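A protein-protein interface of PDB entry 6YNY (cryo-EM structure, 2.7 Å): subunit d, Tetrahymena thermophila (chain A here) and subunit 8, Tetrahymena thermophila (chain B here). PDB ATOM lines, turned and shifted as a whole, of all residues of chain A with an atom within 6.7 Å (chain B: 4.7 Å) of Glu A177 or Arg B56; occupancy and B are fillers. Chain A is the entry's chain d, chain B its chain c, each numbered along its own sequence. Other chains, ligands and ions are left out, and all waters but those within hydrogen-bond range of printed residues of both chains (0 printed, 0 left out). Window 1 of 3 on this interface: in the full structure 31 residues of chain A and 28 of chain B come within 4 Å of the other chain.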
ATOM      1  N   PHE A 171       5.373  12.609 -32.832  1.00  0.00           N
ATOM      2  CA  PHE A 171       6.148  13.180 -31.736  1.00  0.00           C
ATOM      3  C   PHE A 171       5.581  12.717 -30.396  1.00  0.00           C
ATOM      4  O   PHE A 171       5.149  13.500 -29.553  1.00  0.00           O
ATOM      5  CB  PHE A 171       6.161  14.698 -31.846  1.00  0.00           C
ATOM      6  CG  PHE A 171       6.764  15.201 -33.117  1.00  0.00           C
ATOM      7  CD1 PHE A 171       8.080  15.604 -33.158  1.00  0.00           C
ATOM      8  CD2 PHE A 171       6.018  15.259 -34.275  1.00  0.00           C
ATOM      9  CE1 PHE A 171       8.637  16.060 -34.323  1.00  0.00           C
ATOM     10  CE2 PHE A 171       6.571  15.712 -35.441  1.00  0.00           C
ATOM     11  CZ  PHE A 171       7.881  16.114 -35.467  1.00  0.00           C
ATOM     12  N   ARG A 172       5.597  11.400 -30.219  1.00  0.00           N
ATOM     13  CA  ARG A 172       5.064  10.792 -29.013  1.00  0.00           C
ATOM     14  C   ARG A 172       5.716  11.400 -27.781  1.00  0.00           C
ATOM     15  O   ARG A 172       6.942  11.440 -27.666  1.00  0.00           O
ATOM     16  CB  ARG A 172       5.292   9.285 -29.051  1.00  0.00           C
ATOM     17  CG  ARG A 172       4.590   8.521 -27.960  1.00  0.00           C
ATOM     18  CD  ARG A 172       4.978   7.069 -28.004  1.00  0.00           C
ATOM     19  NE  ARG A 172       4.282   6.271 -27.008  1.00  0.00           N
ATOM     20  CZ  ARG A 172       4.595   5.014 -26.720  1.00  0.00           C
ATOM     21  NH1 ARG A 172       5.598   4.422 -27.350  1.00  0.00           N
ATOM     22  NH2 ARG A 172       3.910   4.353 -25.802  1.00  0.00           N
ATOM     23  N   GLY A 173       4.880  11.876 -26.856  1.00  0.00           N
ATOM     24  CA  GLY A 173       5.323  12.576 -25.665  1.00  0.00           C
ATOM     25  C   GLY A 173       4.770  13.983 -25.556  1.00  0.00           C
ATOM     26  O   GLY A 173       4.658  14.516 -24.448  1.00  0.00           O
ATOM     27  N   LEU A 174       4.426  14.597 -26.689  1.00  0.00           N
ATOM     28  CA  LEU A 174       3.842  15.930 -26.657  1.00  0.00           C
ATOM     29  C   LEU A 174       2.438  15.911 -26.068  1.00  0.00           C
ATOM     30  O   LEU A 174       2.043  16.845 -25.362  1.00  0.00           O
ATOM     31  CB  LEU A 174       3.819  16.525 -28.062  1.00  0.00           C
ATOM     32  CG  LEU A 174       5.170  16.874 -28.674  1.00  0.00           C
ATOM     33  CD1 LEU A 174       4.953  17.439 -30.056  1.00  0.00           C
ATOM     34  CD2 LEU A 174       5.929  17.856 -27.816  1.00  0.00           C
ATOM     35  N   GLU A 175       1.666  14.863 -26.354  1.00  0.00           N
ATOM     36  CA  GLU A 175       0.340  14.749 -25.759  1.00  0.00           C
ATOM     37  C   GLU A 175       0.434  14.642 -24.245  1.00  0.00           C
ATOM     38  O   GLU A 175      -0.338  15.277 -23.520  1.00  0.00           O
ATOM     39  CB  GLU A 175      -0.391  13.543 -26.341  1.00  0.00           C
ATOM     40  CG  GLU A 175      -1.842  13.451 -25.933  1.00  0.00           C
ATOM     41  CD  GLU A 175      -2.572  12.314 -26.613  1.00  0.00           C
ATOM     42  OE1 GLU A 175      -1.918  11.531 -27.333  1.00  0.00           O
ATOM     43  OE2 GLU A 175      -3.802  12.204 -26.432  1.00  0.00           O
ATOM     44  N   THR A 176       1.387  13.854 -23.751  1.00  0.00           N
ATOM     45  CA  THR A 176       1.592  13.744 -22.312  1.00  0.00           C
ATOM     46  C   THR A 176       1.978  15.088 -21.708  1.00  0.00           C
ATOM     47  O   THR A 176       1.446  15.489 -20.668  1.00  0.00           O
ATOM     48  CB  THR A 176       2.662  12.692 -22.029  1.00  0.00           C
ATOM     49  OG1 THR A 176       2.267  11.447 -22.613  1.00  0.00           O
ATOM     50  CG2 THR A 176       2.854  12.504 -20.550  1.00  0.00           C
ATOM     51  N   GLU A 177       2.903  15.802 -22.350  1.00  0.00           N
ATOM     52  CA  GLU A 177       3.270  17.126 -21.866  1.00  0.00           C
ATOM     53  C   GLU A 177       2.085  18.079 -21.928  1.00  0.00           C
ATOM     54  O   GLU A 177       1.879  18.888 -21.018  1.00  0.00           O
ATOM     55  CB  GLU A 177       4.433  17.674 -22.686  1.00  0.00           C
ATOM     56  CG  GLU A 177       5.720  16.897 -22.544  1.00  0.00           C
ATOM     57  CD  GLU A 177       6.742  17.267 -23.597  1.00  0.00           C
ATOM     58  OE1 GLU A 177       6.524  18.264 -24.314  1.00  0.00           O
ATOM     59  OE2 GLU A 177       7.761  16.557 -23.712  1.00  0.00           O
ATOM     60  N   LEU A 178       1.296  17.997 -22.998  1.00  0.00           N
ATOM     61  CA  LEU A 178       0.130  18.858 -23.133  1.00  0.00           C
ATOM     62  C   LEU A 178      -0.923  18.542 -22.080  1.00  0.00           C
ATOM     63  O   LEU A 178      -1.664  19.437 -21.658  1.00  0.00           O
ATOM     64  CB  LEU A 178      -0.451  18.712 -24.536  1.00  0.00           C
ATOM     65  CG  LEU A 178      -1.544  19.685 -24.953  1.00  0.00           C
ATOM     66  CD1 LEU A 178      -0.976  21.074 -25.105  1.00  0.00           C
ATOM     67  CD2 LEU A 178      -2.175  19.221 -26.242  1.00  0.00           C
ATOM     68  N   GLU A 179      -1.006  17.285 -21.648  1.00  0.00           N
ATOM     69  CA  GLU A 179      -1.929  16.927 -20.578  1.00  0.00           C
ATOM     70  C   GLU A 179      -1.466  17.482 -19.239  1.00  0.00           C
ATOM     71  O   GLU A 179      -2.283  17.933 -18.431  1.00  0.00           O
ATOM     72  CB  GLU A 179      -2.072  15.410 -20.503  1.00  0.00           C
ATOM     73  CG  GLU A 179      -2.779  14.787 -21.678  1.00  0.00           C
ATOM     74  CD  GLU A 179      -2.640  13.280 -21.707  1.00  0.00           C
ATOM     75  OE1 GLU A 179      -2.264  12.697 -20.672  1.00  0.00           O
ATOM     76  OE2 GLU A 179      -2.899  12.679 -22.769  1.00  0.00           O
ATOM     77  N   GLU A 180      -0.159  17.450 -18.982  1.00  0.00           N
ATOM     78  CA  GLU A 180       0.355  17.970 -17.721  1.00  0.00           C
ATOM     79  C   GLU A 180       0.073  19.459 -17.582  1.00  0.00           C
ATOM     80  O   GLU A 180      -0.273  19.934 -16.494  1.00  0.00           O
ATOM     81  CB  GLU A 180       1.853  17.684 -17.619  1.00  0.00           C
ATOM     82  CG  GLU A 180       2.509  18.192 -16.351  1.00  0.00           C
ATOM     83  CD  GLU A 180       2.974  19.633 -16.446  1.00  0.00           C
ATOM     84  OE1 GLU A 180       3.027  20.178 -17.567  1.00  0.00           O
ATOM     85  OE2 GLU A 180       3.288  20.224 -15.393  1.00  0.00           O
ATOM     86  N   LEU A 181       0.213  20.213 -18.671  1.00  0.00           N
ATOM     87  CA  LEU A 181      -0.118  21.631 -18.631  1.00  0.00           C
ATOM     88  C   LEU A 181      -1.595  21.838 -18.331  1.00  0.00           C
ATOM     89  O   LEU A 181      -1.961  22.728 -17.557  1.00  0.00           O
ATOM     90  CB  LEU A 181       0.250  22.290 -19.956  1.00  0.00           C
ATOM     91  CG  LEU A 181       1.699  22.156 -20.407  1.00  0.00           C
ATOM     92  CD1 LEU A 181       1.847  22.667 -21.819  1.00  0.00           C
ATOM     93  CD2 LEU A 181       2.624  22.896 -19.471  1.00  0.00           C
ATOM     94  N   THR A 182      -2.455  21.020 -18.933  1.00  0.00           N
ATOM     95  CA  THR A 182      -3.890  21.178 -18.741  1.00  0.00           C
ATOM     96  C   THR A 182      -4.306  20.789 -17.328  1.00  0.00           C
ATOM     97  O   THR A 182      -5.100  21.492 -16.694  1.00  0.00           O
ATOM     98  CB  THR A 182      -4.641  20.341 -19.774  1.00  0.00           C
ATOM     99  OG1 THR A 182      -4.198  20.692 -21.090  1.00  0.00           O
ATOM    100  CG2 THR A 182      -6.124  20.570 -19.675  1.00  0.00           C
ATOM    101  N   ASP A 193       8.047  26.942 -21.507  1.00  0.00           N
ATOM    102  CA  ASP A 193       9.041  26.854 -22.566  1.00  0.00           C
ATOM    103  C   ASP A 193      10.064  27.961 -22.363  1.00  0.00           C
ATOM    104  O   ASP A 193       9.708  29.142 -22.315  1.00  0.00           O
ATOM    105  CB  ASP A 193       8.388  26.963 -23.942  1.00  0.00           C
ATOM    106  CG  ASP A 193       7.510  25.775 -24.264  1.00  0.00           C
ATOM    107  OD1 ASP A 193       6.356  25.738 -23.791  1.00  0.00           O
ATOM    108  OD2 ASP A 193       7.974  24.874 -24.990  1.00  0.00           O
ATOM    109  N   HIS B  52       2.652  24.827 -27.980  1.00  0.00           N
ATOM    110  CA  HIS B  52       3.460  23.736 -27.455  1.00  0.00           C
ATOM    111  C   HIS B  52       4.027  22.879 -28.579  1.00  0.00           C
ATOM    112  O   HIS B  52       5.168  22.413 -28.501  1.00  0.00           O
ATOM    113  CB  HIS B  52       2.617  22.890 -26.505  1.00  0.00           C
ATOM    114  CG  HIS B  52       3.379  21.810 -25.814  1.00  0.00           C
ATOM    115  ND1 HIS B  52       3.253  20.481 -26.149  1.00  0.00           N
ATOM    116  CD2 HIS B  52       4.277  21.860 -24.803  1.00  0.00           C
ATOM    117  CE1 HIS B  52       4.040  19.758 -25.375  1.00  0.00           C
ATOM    118  NE2 HIS B  52       4.673  20.571 -24.551  1.00  0.00           N
ATOM    119  N   PHE B  53       3.244  22.666 -29.634  1.00  0.00           N
ATOM    120  CA  PHE B  53       3.694  21.834 -30.743  1.00  0.00           C
ATOM    121  C   PHE B  53       4.803  22.515 -31.533  1.00  0.00           C
ATOM    122  O   PHE B  53       5.756  21.859 -31.967  1.00  0.00           O
ATOM    123  CB  PHE B  53       2.505  21.506 -31.642  1.00  0.00           C
ATOM    124  CG  PHE B  53       2.810  20.522 -32.727  1.00  0.00           C
ATOM    125  CD1 PHE B  53       3.073  19.204 -32.427  1.00  0.00           C
ATOM    126  CD2 PHE B  53       2.805  20.911 -34.053  1.00  0.00           C
ATOM    127  CE1 PHE B  53       3.346  18.300 -33.420  1.00  0.00           C
ATOM    128  CE2 PHE B  53       3.076  20.006 -35.047  1.00  0.00           C
ATOM    129  CZ  PHE B  53       3.345  18.701 -34.731  1.00  0.00           C
ATOM    130  N   PHE B  54       4.698  23.828 -31.729  1.00  0.00           N
ATOM    131  CA  PHE B  54       5.691  24.549 -32.515  1.00  0.00           C
ATOM    132  C   PHE B  54       6.988  24.748 -31.743  1.00  0.00           C
ATOM    133  O   PHE B  54       8.076  24.582 -32.303  1.00  0.00           O
ATOM    134  CB  PHE B  54       5.119  25.894 -32.957  1.00  0.00           C
ATOM    135  CG  PHE B  54       6.109  26.776 -33.641  1.00  0.00           C
ATOM    136  CD1 PHE B  54       6.385  26.616 -34.981  1.00  0.00           C
ATOM    137  CD2 PHE B  54       6.763  27.769 -32.943  1.00  0.00           C
ATOM    138  CE1 PHE B  54       7.293  27.426 -35.608  1.00  0.00           C
ATOM    139  CE2 PHE B  54       7.669  28.578 -33.568  1.00  0.00           C
ATOM    140  CZ  PHE B  54       7.935  28.408 -34.902  1.00  0.00           C
ATOM    141  N   ASN B  55       6.895  25.106 -30.463  1.00  0.00           N
ATOM    142  CA  ASN B  55       8.097  25.417 -29.695  1.00  0.00           C
ATOM    143  C   ASN B  55       8.937  24.172 -29.447  1.00  0.00           C
ATOM    144  O   ASN B  55      10.171  24.228 -29.507  1.00  0.00           O
ATOM    145  CB  ASN B  55       7.721  26.078 -28.373  1.00  0.00           C
ATOM    146  CG  ASN B  55       7.284  27.510 -28.544  1.00  0.00           C
ATOM    147  OD1 ASN B  55       7.583  28.149 -29.551  1.00  0.00           O
ATOM    148  ND2 ASN B  55       6.584  28.029 -27.555  1.00  0.00           N
ATOM    149  N   ARG B  56       8.293  23.046 -29.158  1.00  0.00           N
ATOM    150  CA  ARG B  56       9.002  21.800 -28.901  1.00  0.00           C
ATOM    151  C   ARG B  56       9.594  21.189 -30.158  1.00  0.00           C
ATOM    152  O   ARG B  56      10.261  20.154 -30.063  1.00  0.00           O
ATOM    153  CB  ARG B  56       8.057  20.800 -28.242  1.00  0.00           C
ATOM    154  CG  ARG B  56       7.515  21.256 -26.909  1.00  0.00           C
ATOM    155  CD  ARG B  56       8.537  21.152 -25.797  1.00  0.00           C
ATOM    156  NE  ARG B  56       8.713  19.775 -25.344  1.00  0.00           N
ATOM    157  CZ  ARG B  56       9.666  18.950 -25.761  1.00  0.00           C
ATOM    158  NH1 ARG B  56       9.719  17.722 -25.276  1.00  0.00           N
ATOM    159  NH2 ARG B  56      10.568  19.337 -26.651  1.00  0.00           N
ATOM    160  N   ARG B  57       9.373  21.798 -31.322  1.00  0.00           N
ATOM    161  CA  ARG B  57       9.873  21.281 -32.583  1.00  0.00           C
ATOM    162  C   ARG B  57      10.660  22.297 -33.392  1.00  0.00           C
ATOM    163  O   ARG B  57      11.295  21.908 -34.379  1.00  0.00           O
ATOM    164  CB  ARG B  57       8.708  20.761 -33.440  1.00  0.00           C
ATOM    165  CG  ARG B  57       8.120  19.462 -32.936  1.00  0.00           C
ATOM    166  CD  ARG B  57       6.751  19.169 -33.523  1.00  0.00           C
ATOM    167  NE  ARG B  57       6.732  19.235 -34.980  1.00  0.00           N
ATOM    168  CZ  ARG B  57       6.307  20.276 -35.688  1.00  0.00           C
ATOM    169  NH1 ARG B  57       5.852  21.368 -35.093  1.00  0.00           N
ATOM    170  NH2 ARG B  57       6.337  20.220 -37.007  1.00  0.00           N
ATOM    171  N   HIS B  58      10.651  23.574 -33.012  1.00  0.00           N
ATOM    172  CA  HIS B  58      11.328  24.605 -33.780  1.00  0.00           C
ATOM    173  C   HIS B  58      12.095  25.613 -32.937  1.00  0.00           C
ATOM    174  O   HIS B  58      12.695  26.527 -33.508  1.00  0.00           O
ATOM    175  CB  HIS B  58      10.321  25.367 -34.649  1.00  0.00           C
ATOM    176  CG  HIS B  58       9.791  24.576 -35.802  1.00  0.00           C
ATOM    177  ND1 HIS B  58      10.422  24.536 -37.026  1.00  0.00           N
ATOM    178  CD2 HIS B  58       8.684  23.809 -35.924  1.00  0.00           C
ATOM    179  CE1 HIS B  58       9.730  23.771 -37.850  1.00  0.00           C
ATOM    180  NE2 HIS B  58       8.671  23.316 -37.206  1.00  0.00           N
ATOM    181  N   SER B  59      12.099  25.488 -31.614  1.00  0.00           N
ATOM    182  CA  SER B  59      12.719  26.485 -30.755  1.00  0.00           C
ATOM    183  C   SER B  59      14.173  26.183 -30.425  1.00  0.00           C
ATOM    184  O   SER B  59      14.858  27.056 -29.880  1.00  0.00           O
ATOM    185  CB  SER B  59      11.932  26.623 -29.450  1.00  0.00           C
ATOM    186  OG  SER B  59      12.055  25.462 -28.647  1.00  0.00           O
ATOM    187  N   ARG B  66      20.068  21.769 -25.699  1.00  0.00           N
ATOM    188  CA  ARG B  66      18.715  21.263 -25.526  1.00  0.00           C
ATOM    189  C   ARG B  66      18.762  20.135 -24.504  1.00  0.00           C
ATOM    190  O   ARG B  66      19.420  19.115 -24.727  1.00  0.00           O
ATOM    191  CB  ARG B  66      18.137  20.777 -26.853  1.00  0.00           C
ATOM    192  CG  ARG B  66      16.724  20.248 -26.749  1.00  0.00           C
ATOM    193  CD  ARG B  66      16.243  19.665 -28.054  1.00  0.00           C
ATOM    194  NE  ARG B  66      14.998  18.926 -27.882  1.00  0.00           N
ATOM    195  CZ  ARG B  66      14.478  18.113 -28.793  1.00  0.00           C
ATOM    196  NH1 ARG B  66      15.092  17.925 -29.951  1.00  0.00           N
ATOM    197  NH2 ARG B  66      13.341  17.483 -28.543  1.00  0.00           N
ATOM    198  N   THR B  69      13.800  16.025 -21.595  1.00  0.00           N
ATOM    199  CA  THR B  69      12.669  16.102 -20.687  1.00  0.00           C
ATOM    200  C   THR B  69      12.362  14.723 -20.111  1.00  0.00           C
ATOM    201  O   THR B  69      12.976  13.716 -20.469  1.00  0.00           O
ATOM    202  CB  THR B  69      11.447  16.674 -21.397  1.00  0.00           C
ATOM    203  OG1 THR B  69      11.078  15.824 -22.488  1.00  0.00           O
ATOM    204  CG2 THR B  69      11.736  18.060 -21.920  1.00  0.00           C
ATOM    205  N   THR B  71       9.643  12.835 -20.530  1.00  0.00           N
ATOM    206  CA  THR B  71       9.129  11.938 -21.555  1.00  0.00           C
ATOM    207  C   THR B  71      10.234  11.471 -22.490  1.00  0.00           C
ATOM    208  O   THR B  71      10.261  10.304 -22.898  1.00  0.00           O
ATOM    209  CB  THR B  71       8.023  12.630 -22.343  1.00  0.00           C
ATOM    210  OG1 THR B  71       8.514  13.867 -22.869  1.00  0.00           O
ATOM    211  CG2 THR B  71       6.836  12.893 -21.449  1.00  0.00           C
ATOM    212  N   GLU B  72      11.157  12.364 -22.839  1.00  0.00           N
ATOM    213  CA  GLU B  72      12.252  11.989 -23.721  1.00  0.00           C
ATOM    214  C   GLU B  72      13.220  11.023 -23.053  1.00  0.00           C
ATOM    215  O   GLU B  72      13.942  10.307 -23.752  1.00  0.00           O
ATOM    216  CB  GLU B  72      12.989  13.241 -24.189  1.00  0.00           C
ATOM    217  CG  GLU B  72      12.137  14.180 -25.013  1.00  0.00           C
ATOM    218  CD  GLU B  72      12.831  15.486 -25.327  1.00  0.00           C
ATOM    219  OE1 GLU B  72      13.936  15.720 -24.799  1.00  0.00           O
ATOM    220  OE2 GLU B  72      12.266  16.282 -26.102  1.00  0.00           O
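The guanidinium group of Arg B56 is in salt-bridge range of the side-chain carboxylate of Glu B72 (3.0 Å).
O of Asn B55 sits at hydrogen-bond distance from OG of Ser B59, at 2.4 Å.
The guanidinium group (NH1) of Arg B57 sits close to the backbone carbonyl oxygen (O) of Phe B53 (3.2 Å).
The side-chain hydroxyl of Thr B69 sits at hydrogen-bond distance from the side-chain hydroxyl of Thr B71 (3.2 Å).
N of Thr B69 sits at hydrogen-bond distance from OE1 of Glu B72 (3.2 Å).
Among the printed residues, pairs that only touch across the chains: Phe A171 with Arg B57, Leu A174 with His B52, Leu A174 with Phe B53, Leu A174 with Arg B56, Glu A177 with Thr B69, Leu A181 with His B52, Asp A193 with Asn B55 and Asp A193 with Arg B56.
OE1 of Glu A177 lies within hydrogen-bond range of NE2 of His B52 (3.0 Å).
The side-chain carboxylate of Glu A177 lies within salt-bridge range of the guanidinium group of Arg B56 (2.8 Å).
The side-chain hydroxyl (OG1) of Thr B71 sits at hydrogen-bond distance from the side-chain carboxylate (OE2) of Glu A177.
Of the printed residues of chain B, Glu A177 touches His B52 (3.0 Å), Arg B56 (2.8 Å), Thr B69 (3.6 Å) and Thr B71 (2.9 Å).
Arg B56 touches just these residues of chain A: Leu A174, Glu A177 and Asp A193.
Printed residues of chain B within 4 Å of Asp A193: Asn B55 (3.6 Å) and Arg B56 (3.8 Å).
Of the printed residues of chain A, Thr B71 touches Glu A177.
Of the printed residues of chain B, Leu A174 touches His B52, Phe B53 and Arg B56.
Arg A172 touches none of the printed residues of chain B.
The nearest printed residue of chain B that does not touch Leu A174 is Arg B57 (4.3 Å).
Printed residues of chain A that touch a printed residue of chain B: Phe A171, Leu A174, Glu A177, Leu A181 and Asp A193.
Hydrophobic or aromatic side chains of chain A within 4 Å of the printed part of chain B: Phe A171, Leu A174 and Leu A181.
Hydrophobic or aromatic side chains of chain B within 4 Å of the printed part of chain A: His B52 and Phe B53.
Along chain B the printed residues that touch a printed residue of chain A span positions 52 to 71.
Among the printed residues, 11 pairs touch across the chains.
Among the printed residues, Asp or Glu carboxylates within 4 Å of a Lys or Arg side-chain nitrogen of the other chain: Glu A177 with Arg B56 (2.8 Å).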
